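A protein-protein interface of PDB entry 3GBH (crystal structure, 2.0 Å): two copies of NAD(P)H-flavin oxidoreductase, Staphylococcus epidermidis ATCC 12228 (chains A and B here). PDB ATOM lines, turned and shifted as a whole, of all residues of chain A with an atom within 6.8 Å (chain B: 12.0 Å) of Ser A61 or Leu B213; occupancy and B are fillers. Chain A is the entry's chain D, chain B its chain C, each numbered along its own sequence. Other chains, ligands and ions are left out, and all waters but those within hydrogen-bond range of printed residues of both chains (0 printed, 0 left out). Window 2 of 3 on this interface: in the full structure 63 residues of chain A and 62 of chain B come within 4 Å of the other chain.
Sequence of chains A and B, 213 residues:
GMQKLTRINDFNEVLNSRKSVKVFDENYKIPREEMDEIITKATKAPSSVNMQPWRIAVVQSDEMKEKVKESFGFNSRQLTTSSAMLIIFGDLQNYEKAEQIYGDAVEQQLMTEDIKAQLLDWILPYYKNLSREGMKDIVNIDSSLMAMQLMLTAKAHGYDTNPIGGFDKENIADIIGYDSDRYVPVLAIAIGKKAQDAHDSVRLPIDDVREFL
O of Val B209 lies within hydrogen-bond range of N of Ile A56 (2.7 Å).
N of Glu B211 is in hydrogen-bond range of O of Ile A56 (3.0 Å).
The backbone NH (N) of Val A58 sits at hydrogen-bond distance from the backbone carbonyl oxygen (O) of Glu B211, at 2.8 Å.
OE2 of Glu B211 is in hydrogen-bond range of OH of Tyr A178, at 2.5 Å.
The backbone carbonyl oxygen of Val A58 is in hydrogen-bond range of the backbone NH of Leu B213, at 2.8 Å.
OXT of Leu B213 is in hydrogen-bond range of N of Gln A60, at 2.9 Å.
OG of Ser A61 sits at hydrogen-bond distance from O of Leu B213 (2.5 Å).
The side-chain carboxylate (OD1) of Asp B207 is in salt-bridge range of the guanidinium group (NH1) of Arg B210 (2.8 Å).
The guanidinium group of Arg A32 sits at hydrogen-bond distance from the side-chain amide oxygen of Gln A60 (3.4 Å).
OG of Ser A61 lies within hydrogen-bond range of N of Met A64, at 3.0 Å.
Phe B212 touches Arg A32.
Ile A56 touches Arg B210.
Glu B211 touches Ala A57.
Ala A57 touches Leu B213 (CB to CD1, 3.8 Å).
Phe B212 touches Val A58 (CA to O, 3.5 Å).
Val A59 touches Leu B213.
Gln A60 touches Phe B212.
Met A64 touches Leu B213.
Of chain B, only Leu B213 (2.5 Å) comes within 4 Å of Ser A61.
Leu B213 touches just these residues of chain A: Ala A57 (3.8 Å), Val A58 (2.8 Å), Val A59 (3.8 Å), Gln A60 (2.9 Å), Ser A61 (2.5 Å) and Met A64 (3.6 Å).
Of chain B, only Leu B213 comes within 4 Å of Val A59.
Of chain B, only Phe B212 (3.7 Å) and Leu B213 (2.9 Å) come within 4 Å of Gln A60.
No residue of chain B comes within 4 Å of Glu A63.
Of chain B, only Leu B213 comes within 4 Å of Met A64.
Lys A65 touches none of the printed residues of chain B.
Of the printed residues of chain A, Arg B210 touches Ile A56.
Of the printed residues of chain A, Val B209 touches Ile A56.
Ile B206 touches none of the printed residues of chain A.
Glu A66 touches none of the printed residues of chain B.
Hydrophobic or aromatic side chains of chain A within 4 Å of the printed part of chain B: Ile A56, Ala A57, Val A58, Met A64 and Tyr A178.
Along chain A the printed residues that touch a printed residue of chain B span positions 32 to 178.
Of the 7 printed residues of chain B, 5 touch a printed residue of chain A.
Along chain B the printed residues that touch a printed residue of chain A span positions 209 to 213.
Among the printed residues, 15 pairs touch across the chains.
Among the printed residues, no Asp or Glu carboxylate lies within 4 Å of a Lys or Arg side-chain nitrogen of the other chain.
No position is printed for both chains.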
ATOM      1  N   ARG A  32     -31.071  25.002 -16.748  1.00  0.00           N
ATOM      2  CA  ARG A  32     -31.406  24.512 -18.089  1.00  0.00           C
ATOM      3  C   ARG A  32     -32.506  25.349 -18.700  1.00  0.00           C
ATOM      4  O   ARG A  32     -32.519  25.569 -19.882  1.00  0.00           O
ATOM      5  CB  ARG A  32     -31.948  23.076 -18.080  1.00  0.00           C
ATOM      6  CG  ARG A  32     -30.989  22.006 -17.654  1.00  0.00           C
ATOM      7  CD  ARG A  32     -30.006  21.670 -18.726  1.00  0.00           C
ATOM      8  NE  ARG A  32     -29.200  20.513 -18.350  1.00  0.00           N
ATOM      9  CZ  ARG A  32     -29.587  19.249 -18.514  1.00  0.00           C
ATOM     10  NH1 ARG A  32     -30.786  18.949 -19.027  1.00  0.00           N
ATOM     11  NH2 ARG A  32     -28.774  18.269 -18.143  1.00  0.00           N
ATOM     12  N   ILE A  56     -26.486  22.470 -31.754  1.00  0.00           N
ATOM     13  CA  ILE A  56     -25.664  22.874 -30.610  1.00  0.00           C
ATOM     14  C   ILE A  56     -25.450  21.728 -29.619  1.00  0.00           C
ATOM     15  O   ILE A  56     -26.412  21.167 -29.105  1.00  0.00           O
ATOM     16  CB  ILE A  56     -26.316  24.060 -29.857  1.00  0.00           C
ATOM     17  CG1 ILE A  56     -26.610  25.181 -30.832  1.00  0.00           C
ATOM     18  CG2 ILE A  56     -25.408  24.569 -28.689  1.00  0.00           C
ATOM     19  CD1 ILE A  56     -27.412  26.332 -30.186  1.00  0.00           C
ATOM     20  N   ALA A  57     -24.187  21.384 -29.375  1.00  0.00           N
ATOM     21  CA  ALA A  57     -23.796  20.477 -28.287  1.00  0.00           C
ATOM     22  C   ALA A  57     -23.460  21.352 -27.071  1.00  0.00           C
ATOM     23  O   ALA A  57     -22.506  22.148 -27.108  1.00  0.00           O
ATOM     24  CB  ALA A  57     -22.600  19.652 -28.687  1.00  0.00           C
ATOM     25  N   VAL A  58     -24.280  21.250 -26.025  1.00  0.00           N
ATOM     26  CA  VAL A  58     -24.117  22.063 -24.830  1.00  0.00           C
ATOM     27  C   VAL A  58     -23.315  21.206 -23.887  1.00  0.00           C
ATOM     28  O   VAL A  58     -23.859  20.348 -23.176  1.00  0.00           O
ATOM     29  CB  VAL A  58     -25.463  22.475 -24.185  1.00  0.00           C
ATOM     30  CG1 VAL A  58     -25.196  23.428 -23.010  1.00  0.00           C
ATOM     31  CG2 VAL A  58     -26.387  23.136 -25.191  1.00  0.00           C
ATOM     32  N   VAL A  59     -22.007  21.392 -23.930  1.00  0.00           N
ATOM     33  CA  VAL A  59     -21.076  20.577 -23.128  1.00  0.00           C
ATOM     34  C   VAL A  59     -20.941  21.105 -21.704  1.00  0.00           C
ATOM     35  O   VAL A  59     -20.201  22.065 -21.458  1.00  0.00           O
ATOM     36  CB  VAL A  59     -19.693  20.493 -23.799  1.00  0.00           C
ATOM     37  CG1 VAL A  59     -18.724  19.672 -22.930  1.00  0.00           C
ATOM     38  CG2 VAL A  59     -19.867  19.902 -25.235  1.00  0.00           C
ATOM     39  N   GLN A  60     -21.685  20.502 -20.783  1.00  0.00           N
ATOM     40  CA  GLN A  60     -21.689  20.928 -19.382  1.00  0.00           C
ATOM     41  C   GLN A  60     -21.017  19.972 -18.410  1.00  0.00           C
ATOM     42  O   GLN A  60     -20.447  20.401 -17.417  1.00  0.00           O
ATOM     43  CB  GLN A  60     -23.121  21.100 -18.888  1.00  0.00           C
ATOM     44  CG  GLN A  60     -23.934  22.079 -19.614  1.00  0.00           C
ATOM     45  CD  GLN A  60     -25.298  22.270 -18.973  1.00  0.00           C
ATOM     46  OE1 GLN A  60     -25.877  21.325 -18.442  1.00  0.00           O
ATOM     47  NE2 GLN A  60     -25.822  23.503 -19.037  1.00  0.00           N
ATOM     48  N   SER A  61     -21.124  18.672 -18.646  1.00  0.00           N
ATOM     49  CA  SER A  61     -20.597  17.693 -17.695  1.00  0.00           C
ATOM     50  C   SER A  61     -19.066  17.694 -17.658  1.00  0.00           C
ATOM     51  O   SER A  61     -18.422  17.972 -18.663  1.00  0.00           O
ATOM     52  CB  SER A  61     -21.121  16.294 -18.039  1.00  0.00           C
ATOM     53  OG  SER A  61     -20.525  15.770 -19.207  1.00  0.00           O
ATOM     54  N   ASP A  62     -18.494  17.363 -16.502  1.00  0.00           N
ATOM     55  CA  ASP A  62     -17.050  17.179 -16.380  1.00  0.00           C
ATOM     56  C   ASP A  62     -16.616  16.013 -17.278  1.00  0.00           C
ATOM     57  O   ASP A  62     -15.524  16.028 -17.825  1.00  0.00           O
ATOM     58  CB  ASP A  62     -16.669  16.895 -14.929  1.00  0.00           C
ATOM     59  CG  ASP A  62     -16.569  18.163 -14.091  1.00  0.00           C
ATOM     60  OD1 ASP A  62     -16.430  19.242 -14.689  1.00  0.00           O
ATOM     61  OD2 ASP A  62     -16.607  18.066 -12.846  1.00  0.00           O
ATOM     62  N   GLU A  63     -17.494  15.015 -17.396  1.00  0.00           N
ATOM     63  CA  GLU A  63     -17.306  13.859 -18.283  1.00  0.00           C
ATOM     64  C   GLU A  63     -16.975  14.279 -19.712  1.00  0.00           C
ATOM     65  O   GLU A  63     -15.922  13.929 -20.234  1.00  0.00           O
ATOM     66  CB  GLU A  63     -18.561  12.978 -18.290  1.00  0.00           C
ATOM     67  CG  GLU A  63     -18.293  11.535 -18.651  1.00  0.00           C
ATOM     68  CD  GLU A  63     -19.569  10.686 -18.671  1.00  0.00           C
ATOM     69  OE1 GLU A  63     -20.469  10.907 -17.831  1.00  0.00           O
ATOM     70  OE2 GLU A  63     -19.675   9.806 -19.544  1.00  0.00           O
ATOM     71  N   MET A  64     -17.879  15.024 -20.337  1.00  0.00           N
ATOM     72  CA  MET A  64     -17.687  15.434 -21.712  1.00  0.00           C
ATOM     73  C   MET A  64     -16.603  16.498 -21.847  1.00  0.00           C
ATOM     74  O   MET A  64     -15.832  16.468 -22.813  1.00  0.00           O
ATOM     75  CB  MET A  64     -19.020  15.915 -22.337  1.00  0.00           C
ATOM     76  CG  MET A  64     -18.985  16.134 -23.845  1.00  0.00           C
ATOM     77  SD  MET A  64     -18.354  14.561 -24.883  1.00  0.00           S
ATOM     78  CE  MET A  64     -20.019  13.575 -24.982  1.00  0.00           C
ATOM     79  N   LYS A  65     -16.529  17.444 -20.910  1.00  0.00           N
ATOM     80  CA  LYS A  65     -15.462  18.442 -20.945  1.00  0.00           C
ATOM     81  C   LYS A  65     -14.092  17.743 -20.958  1.00  0.00           C
ATOM     82  O   LYS A  65     -13.209  18.126 -21.682  1.00  0.00           O
ATOM     83  CB  LYS A  65     -15.529  19.367 -19.734  1.00  0.00           C
ATOM     84  CG  LYS A  65     -16.571  20.440 -19.787  1.00  0.00           C
ATOM     85  CD  LYS A  65     -16.552  21.255 -18.503  1.00  0.00           C
ATOM     86  CE  LYS A  65     -17.460  22.491 -18.630  1.00  0.00           C
ATOM     87  NZ  LYS A  65     -17.185  23.383 -17.493  1.00  0.00           N
ATOM     88  N   GLU A  66     -13.933  16.718 -20.128  1.00  0.00           N
ATOM     89  CA  GLU A  66     -12.678  16.005 -20.051  1.00  0.00           C
ATOM     90  C   GLU A  66     -12.364  15.316 -21.389  1.00  0.00           C
ATOM     91  O   GLU A  66     -11.212  15.260 -21.786  1.00  0.00           O
ATOM     92  CB  GLU A  66     -12.738  14.977 -18.928  1.00  0.00           C
ATOM     93  CG  GLU A  66     -11.465  14.190 -18.730  1.00  0.00           C
ATOM     94  CD  GLU A  66     -10.301  15.038 -18.202  1.00  0.00           C
ATOM     95  OE1 GLU A  66     -10.510  16.175 -17.709  1.00  0.00           O
ATOM     96  OE2 GLU A  66      -9.173  14.542 -18.287  1.00  0.00           O
ATOM     97  N   SER A  83     -19.687  27.580 -17.471  1.00  0.00           N
ATOM     98  CA  SER A  83     -20.924  26.898 -17.145  1.00  0.00           C
ATOM     99  C   SER A  83     -21.205  25.852 -18.233  1.00  0.00           C
ATOM    100  O   SER A  83     -21.631  24.756 -17.932  1.00  0.00           O
ATOM    101  CB  SER A  83     -22.068  27.905 -17.007  1.00  0.00           C
ATOM    102  OG  SER A  83     -21.841  28.791 -15.907  1.00  0.00           O
ATOM    103  N   ILE A 176     -17.130  13.679 -29.816  1.00  0.00           N
ATOM    104  CA  ILE A 176     -18.420  13.804 -29.159  1.00  0.00           C
ATOM    105  C   ILE A 176     -19.475  12.803 -29.642  1.00  0.00           C
ATOM    106  O   ILE A 176     -20.511  12.683 -29.001  1.00  0.00           O
ATOM    107  CB  ILE A 176     -19.029  15.245 -29.168  1.00  0.00           C
ATOM    108  CG1 ILE A 176     -19.736  15.602 -30.454  1.00  0.00           C
ATOM    109  CG2 ILE A 176     -18.000  16.330 -28.925  1.00  0.00           C
ATOM    110  CD1 ILE A 176     -20.522  16.863 -30.280  1.00  0.00           C
ATOM    111  N   TYR A 178     -20.815  12.622 -33.070  1.00  0.00           N
ATOM    112  CA  TYR A 178     -21.619  13.042 -34.212  1.00  0.00           C
ATOM    113  C   TYR A 178     -20.976  12.548 -35.506  1.00  0.00           C
ATOM    114  O   TYR A 178     -19.770  12.383 -35.569  1.00  0.00           O
ATOM    115  CB  TYR A 178     -21.740  14.559 -34.275  1.00  0.00           C
ATOM    116  CG  TYR A 178     -22.460  15.217 -33.110  1.00  0.00           C
ATOM    117  CD1 TYR A 178     -23.215  14.477 -32.196  1.00  0.00           C
ATOM    118  CD2 TYR A 178     -22.426  16.589 -32.957  1.00  0.00           C
ATOM    119  CE1 TYR A 178     -23.890  15.088 -31.127  1.00  0.00           C
ATOM    120  CE2 TYR A 178     -23.126  17.223 -31.889  1.00  0.00           C
ATOM    121  CZ  TYR A 178     -23.836  16.458 -30.971  1.00  0.00           C
ATOM    122  OH  TYR A 178     -24.497  17.094 -29.923  1.00  0.00           O
ATOM    123  N   ILE B 206     -36.701  23.463 -30.065  1.00  0.00           N
ATOM    124  CA  ILE B 206     -35.412  23.501 -29.403  1.00  0.00           C
ATOM    125  C   ILE B 206     -34.766  22.120 -29.326  1.00  0.00           C
ATOM    126  O   ILE B 206     -33.559  21.988 -29.490  1.00  0.00           O
ATOM    127  CB  ILE B 206     -35.564  24.141 -27.979  1.00  0.00           C
ATOM    128  CG1 ILE B 206     -34.201  24.353 -27.330  1.00  0.00           C
ATOM    129  CG2 ILE B 206     -36.475  23.317 -27.080  1.00  0.00           C
ATOM    130  CD1 ILE B 206     -34.252  25.231 -26.131  1.00  0.00           C
ATOM    131  N   ASP B 207     -35.595  21.105 -29.107  1.00  0.00           N
ATOM    132  CA  ASP B 207     -35.165  19.701 -29.019  1.00  0.00           C
ATOM    133  C   ASP B 207     -34.593  19.164 -30.338  1.00  0.00           C
ATOM    134  O   ASP B 207     -33.849  18.179 -30.322  1.00  0.00           O
ATOM    135  CB  ASP B 207     -36.276  18.778 -28.529  1.00  0.00           C
ATOM    136  CG  ASP B 207     -36.501  18.881 -27.031  1.00  0.00           C
ATOM    137  OD1 ASP B 207     -35.558  19.135 -26.261  1.00  0.00           O
ATOM    138  OD2 ASP B 207     -37.638  18.705 -26.615  1.00  0.00           O
ATOM    139  N   VAL B 209     -32.566  21.100 -32.234  1.00  0.00           N
ATOM    140  CA  VAL B 209     -31.343  21.843 -32.498  1.00  0.00           C
ATOM    141  C   VAL B 209     -30.279  21.794 -31.414  1.00  0.00           C
ATOM    142  O   VAL B 209     -29.141  22.103 -31.706  1.00  0.00           O
ATOM    143  CB  VAL B 209     -31.598  23.355 -32.834  1.00  0.00           C
ATOM    144  CG1 VAL B 209     -32.594  23.535 -33.993  1.00  0.00           C
ATOM    145  CG2 VAL B 209     -32.080  24.097 -31.635  1.00  0.00           C
ATOM    146  N   ARG B 210     -30.605  21.430 -30.172  1.00  0.00           N
ATOM    147  CA  ARG B 210     -29.577  21.406 -29.118  1.00  0.00           C
ATOM    148  C   ARG B 210     -29.721  20.204 -28.209  1.00  0.00           C
ATOM    149  O   ARG B 210     -30.812  19.669 -28.067  1.00  0.00           O
ATOM    150  CB  ARG B 210     -29.665  22.692 -28.277  1.00  0.00           C
ATOM    151  CG  ARG B 210     -30.967  22.824 -27.426  1.00  0.00           C
ATOM    152  CD  ARG B 210     -30.858  22.210 -26.070  1.00  0.00           C
ATOM    153  NE  ARG B 210     -32.105  22.263 -25.295  1.00  0.00           N
ATOM    154  CZ  ARG B 210     -33.084  21.374 -25.348  1.00  0.00           C
ATOM    155  NH1 ARG B 210     -33.034  20.343 -26.172  1.00  0.00           N
ATOM    156  NH2 ARG B 210     -34.155  21.531 -24.576  1.00  0.00           N
ATOM    157  N   GLU B 211     -28.617  19.769 -27.617  1.00  0.00           N
ATOM    158  CA  GLU B 211     -28.663  18.760 -26.567  1.00  0.00           C
ATOM    159  C   GLU B 211     -27.600  19.032 -25.520  1.00  0.00           C
ATOM    160  O   GLU B 211     -26.621  19.709 -25.770  1.00  0.00           O
ATOM    161  CB  GLU B 211     -28.523  17.338 -27.139  1.00  0.00           C
ATOM    162  CG  GLU B 211     -27.172  17.091 -27.778  1.00  0.00           C
ATOM    163  CD  GLU B 211     -26.981  15.628 -28.225  1.00  0.00           C
ATOM    164  OE1 GLU B 211     -27.743  14.742 -27.782  1.00  0.00           O
ATOM    165  OE2 GLU B 211     -26.042  15.380 -29.011  1.00  0.00           O
ATOM    166  N   PHE B 212     -27.792  18.460 -24.350  1.00  0.00           N
ATOM    167  CA  PHE B 212     -26.918  18.680 -23.193  1.00  0.00           C
ATOM    168  C   PHE B 212     -26.037  17.463 -23.030  1.00  0.00           C
ATOM    169  O   PHE B 212     -26.533  16.371 -23.013  1.00  0.00           O
ATOM    170  CB  PHE B 212     -27.748  18.906 -21.926  1.00  0.00           C
ATOM    171  CG  PHE B 212     -28.505  20.210 -21.927  1.00  0.00           C
ATOM    172  CD1 PHE B 212     -27.898  21.388 -21.499  1.00  0.00           C
ATOM    173  CD2 PHE B 212     -29.830  20.251 -22.343  1.00  0.00           C
ATOM    174  CE1 PHE B 212     -28.600  22.612 -21.530  1.00  0.00           C
ATOM    175  CE2 PHE B 212     -30.541  21.453 -22.371  1.00  0.00           C
ATOM    176  CZ  PHE B 212     -29.921  22.638 -21.967  1.00  0.00           C
ATOM    177  N   LEU B 213     -24.735  17.677 -22.923  1.00  0.00           N
ATOM    178  CA  LEU B 213     -23.764  16.584 -22.738  1.00  0.00           C
ATOM    179  C   LEU B 213     -22.928  16.745 -21.452  1.00  0.00           C
ATOM    180  O   LEU B 213     -22.355  15.763 -20.940  1.00  0.00           O
ATOM    181  CB  LEU B 213     -22.820  16.548 -23.946  1.00  0.00           C
ATOM    182  CG  LEU B 213     -23.471  16.441 -25.335  1.00  0.00           C
ATOM    183  CD1 LEU B 213     -22.404  16.585 -26.383  1.00  0.00           C
ATOM    184  CD2 LEU B 213     -24.194  15.150 -25.521  1.00  0.00           C
ATOM    185  OXT LEU B 213     -22.754  17.853 -20.903  1.00  0.00           O
